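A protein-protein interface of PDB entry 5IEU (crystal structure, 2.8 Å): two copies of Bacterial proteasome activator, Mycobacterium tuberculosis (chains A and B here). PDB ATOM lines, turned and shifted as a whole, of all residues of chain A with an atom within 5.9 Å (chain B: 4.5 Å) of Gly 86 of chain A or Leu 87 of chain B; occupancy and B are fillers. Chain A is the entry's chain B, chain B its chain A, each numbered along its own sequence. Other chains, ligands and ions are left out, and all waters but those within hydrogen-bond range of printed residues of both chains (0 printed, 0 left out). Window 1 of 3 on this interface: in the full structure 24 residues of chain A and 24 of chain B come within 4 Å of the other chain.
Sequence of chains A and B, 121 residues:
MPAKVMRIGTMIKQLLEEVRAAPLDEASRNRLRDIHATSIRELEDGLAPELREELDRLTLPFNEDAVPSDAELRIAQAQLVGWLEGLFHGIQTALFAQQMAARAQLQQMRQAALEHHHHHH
The backbone carbonyl oxygen of Glu 85 of chain B is in hydrogen-bond range of a ring nitrogen (ND1) of His 89 of chain B (3.3 Å). O of Glu 85 of chain A sits at hydrogen-bond distance from ND1 of His 89 of chain A (3.2 Å).
Of the printed residues of chain B, Gly 82 of chain A touches Trp 83. Of the printed residues of chain B, Trp 83 of chain A touches Trp 83 (3.8 Å), Glu 85 (3.9 Å) and Gly 86 (3.5 Å). Of the printed residues of chain B, Leu 87 of chain A touches Gly 86, Leu 87 and Gly 90. Phe 88 of chain A touches none of the printed residues of chain B. Ile 12 of chain B touches none of the printed residues of chain A. Of the printed residues of chain A, Gly 86 of chain B touches Trp 83, Gly 86 and Leu 87. Of the printed residues of chain A, Leu 87 of chain B touches Gly 86, Leu 87, His 89 and Gly 90. Of the printed residues of chain A, Ile 91 of chain B touches Gly 90 and Ile 91. The nearest printed residue of chain B that does not touch Gly 86 of chain A is Gly 90 of chain B (4.9 Å). The nearest residue of chain A that does not touch Leu 87 of chain B is Glu 85 of chain A (5.0 Å).
Among the printed residues, pairs that only touch across the chains: Trp 83 of chain A with Trp 83 of chain B, Trp 83 of chain A with Glu 85 of chain B, Trp 83 of chain A with Gly 86 of chain B, Glu 85 of chain A with Trp 83 of chain B, Gly 86 of chain A with Trp 83 of chain B, Leu 87 of chain A with Leu 87 of chain B, Leu 87 of chain A with Gly 90 of chain B, His 89 of chain A with Trp 83 of chain B, His 89 of chain A with Leu 87 of chain B, Gly 90 of chain A with Leu 87 of chain B, Gly 90 of chain A with Gly 90 of chain B, Gly 90 of chain A with Ile 91 of chain B, Ile 91 of chain A with Gly 90 of chain B and Ile 91 of chain A with Ile 91 of chain B.
Of the 11 printed residues of chain A, 8 touch a printed residue of chain B. Printed residues of chain A that touch a printed residue of chain B: Gly 82, Trp 83, Glu 85, Gly 86, Leu 87, His 89, Gly 90 and Ile 91. Of the 11 printed residues of chain B, 6 touch a printed residue of chain A.
The backbone carbonyl oxygen (O) of Gly 82 of chain A sits close to the backbone NH (N) of Trp 83 of chain B, 3.5 Å away. The backbone carbonyl oxygen (O) of Gly 86 of chain B is in hydrogen-bond range of the backbone NH (N) of Leu 87 of chain A, 3.2 Å away. N of Leu 87 of chain B sits close to O of Gly 86 of chain A, 3.5 Å away. O of Gly 86 of chain B lies close to O of Gly 86 of chain A (3.4 Å).
Gly 86 of chain B touches its own counterpart, Gly 86 of chain A. Leu 87 of chain A touches its own counterpart, Leu 87 of chain B. Gly 90 of chain A touches Ile 91 of chain B, and with the chains exchanged Ile 91 of chain A touches Gly 90 of chain B. Ile 91 of chain A touches its own counterpart, Ile 91 of chain B. Positions printed for both chains: 83, 84, 85, 86, 87, 88, 89, 90 and 91. Of the 18 pairs that touch across the chains among the printed residues, 15 have their exchanged pair printed and touching as well.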
ATOM      1  N   VAL A  81     -24.213 -15.425  19.273  1.00  0.00           N
ATOM      2  CA  VAL A  81     -24.214 -16.263  18.076  1.00  0.00           C
ATOM      3  C   VAL A  81     -24.396 -15.410  16.808  1.00  0.00           C
ATOM      4  O   VAL A  81     -23.753 -15.629  15.782  1.00  0.00           O
ATOM      5  CB  VAL A  81     -25.410 -17.247  18.107  1.00  0.00           C
ATOM      6  CG1 VAL A  81     -25.405 -18.152  16.854  1.00  0.00           C
ATOM      7  CG2 VAL A  81     -25.442 -18.039  19.435  1.00  0.00           C
ATOM      8  N   GLY A  82     -25.352 -14.489  16.883  1.00  0.00           N
ATOM      9  CA  GLY A  82     -25.625 -13.556  15.794  1.00  0.00           C
ATOM     10  C   GLY A  82     -24.476 -12.584  15.591  1.00  0.00           C
ATOM     11  O   GLY A  82     -24.077 -12.302  14.463  1.00  0.00           O
ATOM     12  N   TRP A  83     -23.936 -12.068  16.690  1.00  0.00           N
ATOM     13  CA  TRP A  83     -22.804 -11.146  16.612  1.00  0.00           C
ATOM     14  C   TRP A  83     -21.647 -11.744  15.815  1.00  0.00           C
ATOM     15  O   TRP A  83     -21.101 -11.096  14.903  1.00  0.00           O
ATOM     16  CB  TRP A  83     -22.383 -10.767  18.014  1.00  0.00           C
ATOM     17  CG  TRP A  83     -20.994 -10.254  18.145  1.00  0.00           C
ATOM     18  CD1 TRP A  83     -19.908 -10.938  18.613  1.00  0.00           C
ATOM     19  CD2 TRP A  83     -20.536  -8.927  17.845  1.00  0.00           C
ATOM     20  NE1 TRP A  83     -18.804 -10.125  18.621  1.00  0.00           N
ATOM     21  CE2 TRP A  83     -19.151  -8.883  18.155  1.00  0.00           C
ATOM     22  CE3 TRP A  83     -21.153  -7.777  17.330  1.00  0.00           C
ATOM     23  CZ2 TRP A  83     -18.361  -7.730  17.950  1.00  0.00           C
ATOM     24  CZ3 TRP A  83     -20.357  -6.608  17.142  1.00  0.00           C
ATOM     25  CH2 TRP A  83     -18.984  -6.606  17.452  1.00  0.00           C
ATOM     26  N   LEU A  84     -21.307 -12.989  16.152  1.00  0.00           N
ATOM     27  CA  LEU A  84     -20.207 -13.713  15.497  1.00  0.00           C
ATOM     28  C   LEU A  84     -20.524 -14.077  14.036  1.00  0.00           C
ATOM     29  O   LEU A  84     -19.631 -14.014  13.185  1.00  0.00           O
ATOM     30  CB  LEU A  84     -19.826 -14.966  16.301  1.00  0.00           C
ATOM     31  CG  LEU A  84     -19.136 -14.683  17.651  1.00  0.00           C
ATOM     32  CD1 LEU A  84     -18.503 -15.947  18.178  1.00  0.00           C
ATOM     33  CD2 LEU A  84     -18.065 -13.597  17.591  1.00  0.00           C
ATOM     34  N   GLU A  85     -21.774 -14.455  13.747  1.00  0.00           N
ATOM     35  CA  GLU A  85     -22.215 -14.714  12.370  1.00  0.00           C
ATOM     36  C   GLU A  85     -22.200 -13.430  11.550  1.00  0.00           C
ATOM     37  O   GLU A  85     -21.774 -13.404  10.377  1.00  0.00           O
ATOM     38  CB  GLU A  85     -23.608 -15.310  12.358  1.00  0.00           C
ATOM     39  CG  GLU A  85     -23.596 -16.839  12.375  1.00  0.00           C
ATOM     40  CD  GLU A  85     -24.995 -17.448  12.530  1.00  0.00           C
ATOM     41  OE1 GLU A  85     -25.157 -18.696  12.376  1.00  0.00           O
ATOM     42  OE2 GLU A  85     -25.947 -16.670  12.803  1.00  0.00           O
ATOM     43  N   GLY A  86     -22.644 -12.358  12.192  1.00  0.00           N
ATOM     44  CA  GLY A  86     -22.657 -11.030  11.591  1.00  0.00           C
ATOM     45  C   GLY A  86     -21.271 -10.589  11.171  1.00  0.00           C
ATOM     46  O   GLY A  86     -21.062 -10.246  10.014  1.00  0.00           O
ATOM     47  N   LEU A  87     -20.334 -10.559  12.112  1.00  0.00           N
ATOM     48  CA  LEU A  87     -18.925 -10.254  11.796  1.00  0.00           C
ATOM     49  C   LEU A  87     -18.466 -11.052  10.592  1.00  0.00           C
ATOM     50  O   LEU A  87     -17.886 -10.512   9.673  1.00  0.00           O
ATOM     51  CB  LEU A  87     -17.996 -10.587  12.984  1.00  0.00           C
ATOM     52  CG  LEU A  87     -18.034  -9.731  14.269  1.00  0.00           C
ATOM     53  CD1 LEU A  87     -16.883 -10.168  15.168  1.00  0.00           C
ATOM     54  CD2 LEU A  87     -17.957  -8.228  13.979  1.00  0.00           C
ATOM     55  N   PHE A  88     -18.740 -12.355  10.586  1.00  0.00           N
ATOM     56  CA  PHE A  88     -18.264 -13.209   9.499  1.00  0.00           C
ATOM     57  C   PHE A  88     -18.854 -12.866   8.153  1.00  0.00           C
ATOM     58  O   PHE A  88     -18.145 -12.776   7.168  1.00  0.00           O
ATOM     59  CB  PHE A  88     -18.591 -14.654   9.730  1.00  0.00           C
ATOM     60  CG  PHE A  88     -17.990 -15.532   8.689  1.00  0.00           C
ATOM     61  CD1 PHE A  88     -16.636 -15.827   8.729  1.00  0.00           C
ATOM     62  CD2 PHE A  88     -18.744 -16.003   7.632  1.00  0.00           C
ATOM     63  CE1 PHE A  88     -16.052 -16.642   7.770  1.00  0.00           C
ATOM     64  CE2 PHE A  88     -18.163 -16.790   6.664  1.00  0.00           C
ATOM     65  CZ  PHE A  88     -16.811 -17.116   6.730  1.00  0.00           C
ATOM     66  N   HIS A  89     -20.158 -12.733   8.092  1.00  0.00           N
ATOM     67  CA  HIS A  89     -20.762 -12.339   6.848  1.00  0.00           C
ATOM     68  C   HIS A  89     -20.577 -10.849   6.469  1.00  0.00           C
ATOM     69  O   HIS A  89     -20.563 -10.529   5.275  1.00  0.00           O
ATOM     70  CB  HIS A  89     -22.236 -12.706   6.866  1.00  0.00           C
ATOM     71  CG  HIS A  89     -22.464 -14.179   6.751  1.00  0.00           C
ATOM     72  ND1 HIS A  89     -22.859 -14.950   7.821  1.00  0.00           N
ATOM     73  CD2 HIS A  89     -22.300 -15.034   5.715  1.00  0.00           C
ATOM     74  CE1 HIS A  89     -22.938 -16.214   7.448  1.00  0.00           C
ATOM     75  NE2 HIS A  89     -22.594 -16.295   6.178  1.00  0.00           N
ATOM     76  N   GLY A  90     -20.432  -9.946   7.447  1.00  0.00           N
ATOM     77  CA  GLY A  90     -20.106  -8.529   7.143  1.00  0.00           C
ATOM     78  C   GLY A  90     -18.733  -8.481   6.519  1.00  0.00           C
ATOM     79  O   GLY A  90     -18.498  -7.856   5.494  1.00  0.00           O
ATOM     80  N   ILE A  91     -17.797  -9.167   7.147  1.00  0.00           N
ATOM     81  CA  ILE A  91     -16.421  -9.158   6.660  1.00  0.00           C
ATOM     82  C   ILE A  91     -16.468  -9.773   5.288  1.00  0.00           C
ATOM     83  O   ILE A  91     -15.884  -9.286   4.331  1.00  0.00           O
ATOM     84  CB  ILE A  91     -15.454  -9.979   7.564  1.00  0.00           C
ATOM     85  CG1 ILE A  91     -14.991  -9.167   8.805  1.00  0.00           C
ATOM     86  CG2 ILE A  91     -14.235 -10.422   6.766  1.00  0.00           C
ATOM     87  CD1 ILE A  91     -14.061  -9.954   9.722  1.00  0.00           C
ATOM     88  N   ILE B  12     -28.724  -1.189   7.628  1.00  0.00           N
ATOM     89  CA  ILE B  12     -28.427  -1.782   8.912  1.00  0.00           C
ATOM     90  C   ILE B  12     -28.594  -0.800  10.085  1.00  0.00           C
ATOM     91  O   ILE B  12     -29.277  -1.090  11.065  1.00  0.00           O
ATOM     92  CB  ILE B  12     -26.982  -2.276   8.973  1.00  0.00           C
ATOM     93  CG1 ILE B  12     -26.770  -3.536   8.122  1.00  0.00           C
ATOM     94  CG2 ILE B  12     -26.597  -2.572  10.426  1.00  0.00           C
ATOM     95  CD1 ILE B  12     -25.303  -3.987   8.116  1.00  0.00           C
ATOM     96  N   LEU B  43     -27.419  -8.166   1.443  1.00  0.00           N
ATOM     97  CA  LEU B  43     -26.039  -8.652   1.370  1.00  0.00           C
ATOM     98  C   LEU B  43     -25.813  -9.401   0.101  1.00  0.00           C
ATOM     99  O   LEU B  43     -24.723  -9.358  -0.476  1.00  0.00           O
ATOM    100  CB  LEU B  43     -25.724  -9.596   2.546  1.00  0.00           C
ATOM    101  CG  LEU B  43     -25.754  -9.033   3.974  1.00  0.00           C
ATOM    102  CD1 LEU B  43     -25.401 -10.149   4.927  1.00  0.00           C
ATOM    103  CD2 LEU B  43     -24.805  -7.845   4.168  1.00  0.00           C
ATOM    104  N   TRP B  83     -26.526  -9.881  15.040  1.00  0.00           N
ATOM    105  CA  TRP B  83     -26.406 -10.096  13.612  1.00  0.00           C
ATOM    106  C   TRP B  83     -26.279  -8.789  12.888  1.00  0.00           C
ATOM    107  O   TRP B  83     -25.395  -8.619  12.021  1.00  0.00           O
ATOM    108  CB  TRP B  83     -27.606 -10.872  13.085  1.00  0.00           C
ATOM    109  CG  TRP B  83     -27.691 -10.905  11.577  1.00  0.00           C
ATOM    110  CD1 TRP B  83     -28.596 -10.232  10.762  1.00  0.00           C
ATOM    111  CD2 TRP B  83     -26.830 -11.658  10.650  1.00  0.00           C
ATOM    112  NE1 TRP B  83     -28.362 -10.509   9.439  1.00  0.00           N
ATOM    113  CE2 TRP B  83     -27.319 -11.355   9.303  1.00  0.00           C
ATOM    114  CE3 TRP B  83     -25.750 -12.515  10.798  1.00  0.00           C
ATOM    115  CZ2 TRP B  83     -26.735 -11.899   8.172  1.00  0.00           C
ATOM    116  CZ3 TRP B  83     -25.172 -13.057   9.649  1.00  0.00           C
ATOM    117  CH2 TRP B  83     -25.653 -12.755   8.369  1.00  0.00           C
ATOM    118  N   LEU B  84     -27.153  -7.845  13.224  1.00  0.00           N
ATOM    119  CA  LEU B  84     -27.127  -6.523  12.611  1.00  0.00           C
ATOM    120  C   LEU B  84     -25.865  -5.768  13.008  1.00  0.00           C
ATOM    121  O   LEU B  84     -25.251  -5.086  12.187  1.00  0.00           O
ATOM    122  CB  LEU B  84     -28.368  -5.721  13.010  1.00  0.00           C
ATOM    123  CG  LEU B  84     -29.705  -6.227  12.466  1.00  0.00           C
ATOM    124  CD1 LEU B  84     -30.863  -5.478  13.106  1.00  0.00           C
ATOM    125  CD2 LEU B  84     -29.751  -6.101  10.950  1.00  0.00           C
ATOM    126  N   GLU B  85     -25.479  -5.895  14.274  1.00  0.00           N
ATOM    127  CA  GLU B  85     -24.280  -5.239  14.780  1.00  0.00           C
ATOM    128  C   GLU B  85     -23.025  -5.896  14.215  1.00  0.00           C
ATOM    129  O   GLU B  85     -22.060  -5.217  13.869  1.00  0.00           O
ATOM    130  CB  GLU B  85     -24.252  -5.279  16.309  1.00  0.00           C
ATOM    131  CG  GLU B  85     -25.281  -4.377  16.971  1.00  0.00           C
ATOM    132  CD  GLU B  85     -24.683  -3.071  17.458  1.00  0.00           C
ATOM    133  OE1 GLU B  85     -23.686  -2.613  16.862  1.00  0.00           O
ATOM    134  OE2 GLU B  85     -25.210  -2.503  18.437  1.00  0.00           O
ATOM    135  N   GLY B  86     -23.049  -7.222  14.125  1.00  0.00           N
ATOM    136  CA  GLY B  86     -21.927  -7.970  13.589  1.00  0.00           C
ATOM    137  C   GLY B  86     -21.624  -7.590  12.155  1.00  0.00           C
ATOM    138  O   GLY B  86     -20.468  -7.383  11.787  1.00  0.00           O
ATOM    139  N   LEU B  87     -22.670  -7.494  11.340  1.00  0.00           N
ATOM    140  CA  LEU B  87     -22.519  -7.120   9.940  1.00  0.00           C
ATOM    141  C   LEU B  87     -21.930  -5.720   9.816  1.00  0.00           C
ATOM    142  O   LEU B  87     -21.106  -5.457   8.938  1.00  0.00           O
ATOM    143  CB  LEU B  87     -23.865  -7.190   9.217  1.00  0.00           C
ATOM    144  CG  LEU B  87     -24.512  -8.573   9.121  1.00  0.00           C
ATOM    145  CD1 LEU B  87     -26.000  -8.453   8.835  1.00  0.00           C
ATOM    146  CD2 LEU B  87     -23.823  -9.417   8.058  1.00  0.00           C
ATOM    147  N   PHE B  88     -22.355  -4.825  10.701  1.00  0.00           N
ATOM    148  CA  PHE B  88     -21.859  -3.456  10.703  1.00  0.00           C
ATOM    149  C   PHE B  88     -20.378  -3.385  10.994  1.00  0.00           C
ATOM    150  O   PHE B  88     -19.607  -2.835  10.217  1.00  0.00           O
ATOM    151  CB  PHE B  88     -22.543  -2.635  11.762  1.00  0.00           C
ATOM    152  CG  PHE B  88     -22.270  -1.176  11.623  1.00  0.00           C
ATOM    153  CD1 PHE B  88     -23.066  -0.397  10.783  1.00  0.00           C
ATOM    154  CD2 PHE B  88     -21.211  -0.586  12.268  1.00  0.00           C
ATOM    155  CE1 PHE B  88     -22.819   0.955  10.616  1.00  0.00           C
ATOM    156  CE2 PHE B  88     -20.947   0.752  12.087  1.00  0.00           C
ATOM    157  CZ  PHE B  88     -21.755   1.525  11.266  1.00  0.00           C
ATOM    158  N   HIS B  89     -19.977  -3.950  12.120  1.00  0.00           N
ATOM    159  CA  HIS B  89     -18.570  -3.909  12.472  1.00  0.00           C
ATOM    160  C   HIS B  89     -17.702  -4.833  11.621  1.00  0.00           C
ATOM    161  O   HIS B  89     -16.535  -4.514  11.401  1.00  0.00           O
ATOM    162  CB  HIS B  89     -18.385  -4.175  13.966  1.00  0.00           C
ATOM    163  CG  HIS B  89     -18.877  -3.042  14.822  1.00  0.00           C
ATOM    164  ND1 HIS B  89     -20.216  -2.819  15.061  1.00  0.00           N
ATOM    165  CD2 HIS B  89     -18.211  -2.027  15.429  1.00  0.00           C
ATOM    166  CE1 HIS B  89     -20.353  -1.737  15.809  1.00  0.00           C
ATOM    167  NE2 HIS B  89     -19.153  -1.237  16.044  1.00  0.00           N
ATOM    168  N   GLY B  90     -18.248  -5.956  11.138  1.00  0.00           N
ATOM    169  CA  GLY B  90     -17.504  -6.857  10.209  1.00  0.00           C
ATOM    170  C   GLY B  90     -17.088  -6.081   8.963  1.00  0.00           C
ATOM    171  O   GLY B  90     -15.931  -6.082   8.562  1.00  0.00           O
ATOM    172  N   ILE B  91     -18.037  -5.374   8.367  1.00  0.00           N
ATOM    173  CA  ILE B  91     -17.721  -4.485   7.250  1.00  0.00           C
ATOM    174  C   ILE B  91     -16.677  -3.462   7.661  1.00  0.00           C
ATOM    175  O   ILE B  91     -15.705  -3.240   6.940  1.00  0.00           O
ATOM    176  CB  ILE B  91     -18.974  -3.699   6.765  1.00  0.00           C
ATOM    177  CG1 ILE B  91     -19.940  -4.628   5.987  1.00  0.00           C
ATOM    178  CG2 ILE B  91     -18.550  -2.488   5.926  1.00  0.00           C
ATOM    179  CD1 ILE B  91     -21.403  -4.210   6.047  1.00  0.00           C
